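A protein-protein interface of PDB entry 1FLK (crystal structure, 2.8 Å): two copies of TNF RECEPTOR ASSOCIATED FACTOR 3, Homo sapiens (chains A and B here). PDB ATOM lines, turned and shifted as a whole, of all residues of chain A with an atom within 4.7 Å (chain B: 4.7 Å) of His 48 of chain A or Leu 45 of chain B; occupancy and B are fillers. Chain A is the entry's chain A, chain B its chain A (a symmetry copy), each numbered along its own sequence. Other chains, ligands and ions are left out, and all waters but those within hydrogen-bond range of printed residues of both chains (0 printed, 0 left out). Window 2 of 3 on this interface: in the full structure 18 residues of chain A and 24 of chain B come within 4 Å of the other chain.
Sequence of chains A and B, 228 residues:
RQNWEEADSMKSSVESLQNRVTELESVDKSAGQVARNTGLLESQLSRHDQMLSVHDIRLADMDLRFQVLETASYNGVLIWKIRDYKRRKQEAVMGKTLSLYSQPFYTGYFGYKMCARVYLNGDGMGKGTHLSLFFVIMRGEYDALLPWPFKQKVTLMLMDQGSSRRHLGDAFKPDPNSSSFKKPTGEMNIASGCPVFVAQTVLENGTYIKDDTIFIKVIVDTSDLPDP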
ATOM      1  N   LEU A  41     -11.306  -0.847  10.931  1.00  0.00           N
ATOM      2  CA  LEU A  41     -10.157   0.030  10.682  1.00  0.00           C
ATOM      3  C   LEU A  41      -9.161  -0.707   9.783  1.00  0.00           C
ATOM      4  O   LEU A  41      -8.751  -0.206   8.727  1.00  0.00           O
ATOM      5  CB  LEU A  41      -9.438   0.399  11.991  1.00  0.00           C
ATOM      6  CG  LEU A  41      -9.924   1.348  13.106  1.00  0.00           C
ATOM      7  CD1 LEU A  41     -10.522   2.611  12.490  1.00  0.00           C
ATOM      8  CD2 LEU A  41     -10.907   0.650  14.020  1.00  0.00           C
ATOM      9  N   GLN A  44     -10.289  -1.403   6.194  1.00  0.00           N
ATOM     10  CA  GLN A  44     -10.194  -0.182   5.415  1.00  0.00           C
ATOM     11  C   GLN A  44      -8.733   0.044   5.106  1.00  0.00           C
ATOM     12  O   GLN A  44      -8.379   0.423   3.989  1.00  0.00           O
ATOM     13  CB  GLN A  44     -10.790   0.997   6.179  1.00  0.00           C
ATOM     14  CG  GLN A  44     -12.310   0.922   6.312  1.00  0.00           C
ATOM     15  CD  GLN A  44     -13.004   0.500   5.009  1.00  0.00           C
ATOM     16  OE1 GLN A  44     -12.703   1.029   3.927  1.00  0.00           O
ATOM     17  NE2 GLN A  44     -13.940  -0.459   5.114  1.00  0.00           N
ATOM     18  N   LEU A  45      -7.885  -0.220   6.096  1.00  0.00           N
ATOM     19  CA  LEU A  45      -6.450  -0.082   5.917  1.00  0.00           C
ATOM     20  C   LEU A  45      -5.943  -1.058   4.830  1.00  0.00           C
ATOM     21  O   LEU A  45      -5.086  -0.704   4.004  1.00  0.00           O
ATOM     22  CB  LEU A  45      -5.731  -0.334   7.252  1.00  0.00           C
ATOM     23  CG  LEU A  45      -5.510   0.890   8.156  1.00  0.00           C
ATOM     24  CD1 LEU A  45      -4.944   0.486   9.515  1.00  0.00           C
ATOM     25  CD2 LEU A  45      -4.569   1.832   7.454  1.00  0.00           C
ATOM     26  N   SER A  46      -6.480  -2.279   4.817  1.00  0.00           N
ATOM     27  CA  SER A  46      -6.072  -3.268   3.822  1.00  0.00           C
ATOM     28  C   SER A  46      -6.517  -2.875   2.423  1.00  0.00           C
ATOM     29  O   SER A  46      -5.890  -3.245   1.430  1.00  0.00           O
ATOM     30  CB  SER A  46      -6.648  -4.637   4.153  1.00  0.00           C
ATOM     31  OG  SER A  46      -6.354  -5.545   3.110  1.00  0.00           O
ATOM     32  N   ARG A  47      -7.615  -2.135   2.350  1.00  0.00           N
ATOM     33  CA  ARG A  47      -8.133  -1.685   1.069  1.00  0.00           C
ATOM     34  C   ARG A  47      -7.194  -0.657   0.436  1.00  0.00           C
ATOM     35  O   ARG A  47      -6.805  -0.803  -0.728  1.00  0.00           O
ATOM     36  CB  ARG A  47      -9.530  -1.092   1.249  1.00  0.00           C
ATOM     37  CG  ARG A  47     -10.658  -2.108   1.171  1.00  0.00           C
ATOM     38  CD  ARG A  47     -11.993  -1.479   1.534  1.00  0.00           C
ATOM     39  NE  ARG A  47     -12.107  -0.104   1.048  1.00  0.00           N
ATOM     40  CZ  ARG A  47     -12.196   0.247  -0.231  1.00  0.00           C
ATOM     41  NH1 ARG A  47     -12.195  -0.671  -1.188  1.00  0.00           N
ATOM     42  NH2 ARG A  47     -12.271   1.529  -0.553  1.00  0.00           N
ATOM     43  N   HIS A  48      -6.821   0.367   1.209  1.00  0.00           N
ATOM     44  CA  HIS A  48      -5.926   1.430   0.733  1.00  0.00           C
ATOM     45  C   HIS A  48      -4.506   0.923   0.465  1.00  0.00           C
ATOM     46  O   HIS A  48      -3.765   1.488  -0.347  1.00  0.00           O
ATOM     47  CB  HIS A  48      -5.893   2.573   1.749  1.00  0.00           C
ATOM     48  CG  HIS A  48      -7.248   3.105   2.104  1.00  0.00           C
ATOM     49  ND1 HIS A  48      -8.216   3.364   1.160  1.00  0.00           N
ATOM     50  CD2 HIS A  48      -7.798   3.420   3.301  1.00  0.00           C
ATOM     51  CE1 HIS A  48      -9.304   3.811   1.760  1.00  0.00           C
ATOM     52  NE2 HIS A  48      -9.076   3.855   3.060  1.00  0.00           N
ATOM     53  N   ASP A  49      -4.140  -0.150   1.161  1.00  0.00           N
ATOM     54  CA  ASP A  49      -2.840  -0.786   0.994  1.00  0.00           C
ATOM     55  C   ASP A  49      -2.735  -1.316  -0.450  1.00  0.00           C
ATOM     56  O   ASP A  49      -1.718  -1.118  -1.116  1.00  0.00           O
ATOM     57  CB  ASP A  49      -2.706  -1.927   2.000  1.00  0.00           C
ATOM     58  CG  ASP A  49      -1.317  -2.012   2.612  1.00  0.00           C
ATOM     59  OD1 ASP A  49      -1.221  -2.460   3.783  1.00  0.00           O
ATOM     60  OD2 ASP A  49      -0.330  -1.639   1.934  1.00  0.00           O
ATOM     61  N   GLN A  50      -3.796  -1.967  -0.935  1.00  0.00           N
ATOM     62  CA  GLN A  50      -3.832  -2.502  -2.296  1.00  0.00           C
ATOM     63  C   GLN A  50      -3.867  -1.399  -3.362  1.00  0.00           C
ATOM     64  O   GLN A  50      -3.171  -1.461  -4.382  1.00  0.00           O
ATOM     65  CB  GLN A  50      -5.039  -3.431  -2.444  1.00  0.00           C
ATOM     66  CG  GLN A  50      -4.870  -4.741  -1.682  1.00  0.00           C
ATOM     67  CD  GLN A  50      -6.116  -5.627  -1.675  1.00  0.00           C
ATOM     68  OE1 GLN A  50      -7.086  -5.360  -0.954  1.00  0.00           O
ATOM     69  NE2 GLN A  50      -6.092  -6.694  -2.476  1.00  0.00           N
ATOM     70  N   MET A  51      -4.682  -0.382  -3.108  1.00  0.00           N
ATOM     71  CA  MET A  51      -4.825   0.747  -4.023  1.00  0.00           C
ATOM     72  C   MET A  51      -3.496   1.495  -4.190  1.00  0.00           C
ATOM     73  O   MET A  51      -3.063   1.761  -5.312  1.00  0.00           O
ATOM     74  CB  MET A  51      -5.917   1.679  -3.492  1.00  0.00           C
ATOM     75  CG  MET A  51      -6.362   2.774  -4.446  1.00  0.00           C
ATOM     76  SD  MET A  51      -8.165   2.847  -4.693  1.00  0.00           S
ATOM     77  CE  MET A  51      -8.757   2.816  -2.993  1.00  0.00           C
ATOM     78  N   LEU A  52      -2.849   1.821  -3.070  1.00  0.00           N
ATOM     79  CA  LEU A  52      -1.555   2.525  -3.084  1.00  0.00           C
ATOM     80  C   LEU A  52      -0.541   1.746  -3.925  1.00  0.00           C
ATOM     81  O   LEU A  52       0.242   2.318  -4.702  1.00  0.00           O
ATOM     82  CB  LEU A  52      -1.039   2.710  -1.643  1.00  0.00           C
ATOM     83  CG  LEU A  52      -1.675   3.873  -0.857  1.00  0.00           C
ATOM     84  CD1 LEU A  52      -1.451   3.746   0.631  1.00  0.00           C
ATOM     85  CD2 LEU A  52      -1.107   5.170  -1.382  1.00  0.00           C
ATOM     86  N   LEU B  41      -8.490   7.930  14.014  1.00  0.00           N
ATOM     87  CA  LEU B  41      -8.093   6.896  13.053  1.00  0.00           C
ATOM     88  C   LEU B  41      -8.979   7.012  11.810  1.00  0.00           C
ATOM     89  O   LEU B  41      -8.491   7.119  10.677  1.00  0.00           O
ATOM     90  CB  LEU B  41      -8.274   5.484  13.638  1.00  0.00           C
ATOM     91  CG  LEU B  41      -7.430   4.796  14.732  1.00  0.00           C
ATOM     92  CD1 LEU B  41      -5.946   5.048  14.478  1.00  0.00           C
ATOM     93  CD2 LEU B  41      -7.850   5.258  16.109  1.00  0.00           C
ATOM     94  N   GLU B  42     -10.292   6.993  12.049  1.00  0.00           N
ATOM     95  CA  GLU B  42     -11.313   7.085  11.000  1.00  0.00           C
ATOM     96  C   GLU B  42     -11.190   8.316  10.113  1.00  0.00           C
ATOM     97  O   GLU B  42     -11.266   8.208   8.885  1.00  0.00           O
ATOM     98  CB  GLU B  42     -12.691   7.048  11.643  1.00  0.00           C
ATOM     99  CG  GLU B  42     -12.901   5.796  12.455  1.00  0.00           C
ATOM    100  CD  GLU B  42     -14.196   5.806  13.214  1.00  0.00           C
ATOM    101  OE1 GLU B  42     -14.489   4.799  13.887  1.00  0.00           O
ATOM    102  OE2 GLU B  42     -14.920   6.820  13.141  1.00  0.00           O
ATOM    103  N   SER B  43     -10.995   9.477  10.741  1.00  0.00           N
ATOM    104  CA  SER B  43     -10.846  10.738  10.017  1.00  0.00           C
ATOM    105  C   SER B  43      -9.625  10.652   9.119  1.00  0.00           C
ATOM    106  O   SER B  43      -9.671  11.034   7.943  1.00  0.00           O
ATOM    107  CB  SER B  43     -10.664  11.897  10.991  1.00  0.00           C
ATOM    108  OG  SER B  43     -11.558  11.781  12.083  1.00  0.00           O
ATOM    109  N   GLN B  44      -8.525  10.155   9.674  1.00  0.00           N
ATOM    110  CA  GLN B  44      -7.314  10.026   8.883  1.00  0.00           C
ATOM    111  C   GLN B  44      -7.616   9.077   7.748  1.00  0.00           C
ATOM    112  O   GLN B  44      -7.205   9.307   6.610  1.00  0.00           O
ATOM    113  CB  GLN B  44      -6.156   9.521   9.740  1.00  0.00           C
ATOM    114  CG  GLN B  44      -5.664  10.550  10.755  1.00  0.00           C
ATOM    115  CD  GLN B  44      -5.543  11.962  10.164  1.00  0.00           C
ATOM    116  OE1 GLN B  44      -4.984  12.150   9.073  1.00  0.00           O
ATOM    117  NE2 GLN B  44      -6.070  12.962  10.892  1.00  0.00           N
ATOM    118  N   LEU B  45      -8.359   8.020   8.061  1.00  0.00           N
ATOM    119  CA  LEU B  45      -8.754   7.051   7.053  1.00  0.00           C
ATOM    120  C   LEU B  45      -9.635   7.719   5.972  1.00  0.00           C
ATOM    121  O   LEU B  45      -9.493   7.439   4.771  1.00  0.00           O
ATOM    122  CB  LEU B  45      -9.501   5.882   7.716  1.00  0.00           C
ATOM    123  CG  LEU B  45      -8.642   4.700   8.196  1.00  0.00           C
ATOM    124  CD1 LEU B  45      -9.473   3.690   8.983  1.00  0.00           C
ATOM    125  CD2 LEU B  45      -8.024   4.046   6.989  1.00  0.00           C
ATOM    126  N   SER B  46     -10.531   8.613   6.392  1.00  0.00           N
ATOM    127  CA  SER B  46     -11.403   9.305   5.445  1.00  0.00           C
ATOM    128  C   SER B  46     -10.622  10.257   4.555  1.00  0.00           C
ATOM    129  O   SER B  46     -11.018  10.536   3.423  1.00  0.00           O
ATOM    130  CB  SER B  46     -12.480  10.091   6.178  1.00  0.00           C
ATOM    131  OG  SER B  46     -13.226  10.858   5.253  1.00  0.00           O
ATOM    132  N   ARG B  47      -9.517  10.769   5.081  1.00  0.00           N
ATOM    133  CA  ARG B  47      -8.677  11.681   4.323  1.00  0.00           C
ATOM    134  C   ARG B  47      -7.994  10.954   3.165  1.00  0.00           C
ATOM    135  O   ARG B  47      -8.064  11.405   2.017  1.00  0.00           O
ATOM    136  CB  ARG B  47      -7.636  12.320   5.242  1.00  0.00           C
ATOM    137  CG  ARG B  47      -8.108  13.584   5.942  1.00  0.00           C
ATOM    138  CD  ARG B  47      -7.092  14.058   6.967  1.00  0.00           C
ATOM    139  NE  ARG B  47      -5.715  13.847   6.520  1.00  0.00           N
ATOM    140  CZ  ARG B  47      -5.132  14.496   5.519  1.00  0.00           C
ATOM    141  NH1 ARG B  47      -5.788  15.425   4.837  1.00  0.00           N
ATOM    142  NH2 ARG B  47      -3.883  14.201   5.188  1.00  0.00           N
ATOM    143  N   HIS B  48      -7.349   9.822   3.468  1.00  0.00           N
ATOM    144  CA  HIS B  48      -6.645   9.020   2.459  1.00  0.00           C
ATOM    145  C   HIS B  48      -7.601   8.380   1.448  1.00  0.00           C
ATOM    146  O   HIS B  48      -7.227   8.087   0.307  1.00  0.00           O
ATOM    147  CB  HIS B  48      -5.808   7.941   3.146  1.00  0.00           C
ATOM    148  CG  HIS B  48      -4.871   8.475   4.186  1.00  0.00           C
ATOM    149  ND1 HIS B  48      -4.093   9.593   3.982  1.00  0.00           N
ATOM    150  CD2 HIS B  48      -4.591   8.047   5.440  1.00  0.00           C
ATOM    151  CE1 HIS B  48      -3.378   9.833   5.067  1.00  0.00           C
ATOM    152  NE2 HIS B  48      -3.662   8.909   5.966  1.00  0.00           N
ATOM    153  N   ASP B  49      -8.840   8.169   1.885  1.00  0.00           N
ATOM    154  CA  ASP B  49      -9.885   7.609   1.038  1.00  0.00           C
ATOM    155  C   ASP B  49     -10.142   8.581  -0.130  1.00  0.00           C
ATOM    156  O   ASP B  49     -10.233   8.162  -1.284  1.00  0.00           O
ATOM    157  CB  ASP B  49     -11.152   7.411   1.868  1.00  0.00           C
ATOM    158  CG  ASP B  49     -11.874   6.115   1.540  1.00  0.00           C
ATOM    159  OD1 ASP B  49     -12.529   5.563   2.461  1.00  0.00           O
ATOM    160  OD2 ASP B  49     -11.792   5.651   0.378  1.00  0.00           O
ATOM    161  N   LEU B  52      -6.783   8.861  -2.444  1.00  0.00           N
ATOM    162  CA  LEU B  52      -6.641   7.662  -3.288  1.00  0.00           C
ATOM    163  C   LEU B  52      -7.583   7.749  -4.491  1.00  0.00           C
ATOM    164  O   LEU B  52      -7.225   7.404  -5.630  1.00  0.00           O
ATOM    165  CB  LEU B  52      -6.933   6.395  -2.459  1.00  0.00           C
ATOM    166  CG  LEU B  52      -5.779   5.911  -1.561  1.00  0.00           C
ATOM    167  CD1 LEU B  52      -6.250   4.954  -0.492  1.00  0.00           C
ATOM    168  CD2 LEU B  52      -4.728   5.272  -2.437  1.00  0.00           C
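Among the printed residues, merely in contact across the chains: Leu 41 of chain A with Leu 41 of chain B (3.8 Å), Leu 41 of chain A with Glu 42 of chain B (3.98 Å), Leu 41 of chain A with Leu 45 of chain B (3.8 Å), His 48 of chain A with Leu 45 of chain B (3.7 Å), His 48 of chain A with Asp 49 of chain B (3.4 Å), His 48 of chain A with Leu 52 of chain B (3.0 Å), Met 51 of chain A with Leu 52 of chain B (3.6 Å) and Leu 52 of chain A with Leu 52 of chain B (3.7 Å).
His 48 of chain A touches three residues of chain B. Of chain A, only Leu 41 and His 48 come within 4 Å of Leu 45 of chain B. Of the printed residues of chain B, Leu 52 of chain A touches Leu 52. Printed residues of chain B within 4 Å of Met 51 of chain A: Leu 52. Of the printed residues of chain A, Glu 42 of chain B touches Leu 41. Of the printed residues of chain A, Leu 41 of chain B touches Leu 41. Arg 47 of chain B touches none of the printed residues of chain A. Ser 46 of chain A touches none of the printed residues of chain B. The nearest printed residue of chain B that does not touch His 48 of chain A is His 48 of chain B (4.9 Å). The nearest printed residue of chain A that does not touch Leu 45 of chain B is Gln 44 of chain A (4.1 Å). The nearest printed residue of chain A that does not touch Glu 42 of chain B is His 48 of chain A (7.6 Å).
Of the 10 printed residues of chain B, 5 touch a printed residue of chain A. Hydrophobic or aromatic side chains of chain B that line the printed part of chain A: Leu 41, Leu 45 and Leu 52. Of the 10 printed residues of chain A, 4 touch a printed residue of chain B. Printed residues of chain A that touch a printed residue of chain B: Leu 41, His 48, Met 51 and Leu 52. Hydrophobic or aromatic side chains of chain A that line the printed part of chain B: Leu 41, His 48, Met 51 and Leu 52. Among the printed residues, 8 pairs touch across the chains. Among the printed residues, no Asp or Glu carboxylate lies within 4 Å of a Lys or Arg side-chain nitrogen of the other chain.
Leu 41 of chain A touches its own counterpart, Leu 41 of chain B. His 48 of chain A touches Leu 45 of chain B, but with the chains exchanged Leu 45 of chain A does not touch His 48 of chain B (6.5 Å). His 48 of chain A touches Asp 49 of chain B, but with the chains exchanged Asp 49 of chain A does not touch His 48 of chain B (8.5 Å). Leu 52 of chain A touches its own counterpart, Leu 52 of chain B. Positions printed for both chains: 41, 44, 45, 46, 47, 48, 49 and 52.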
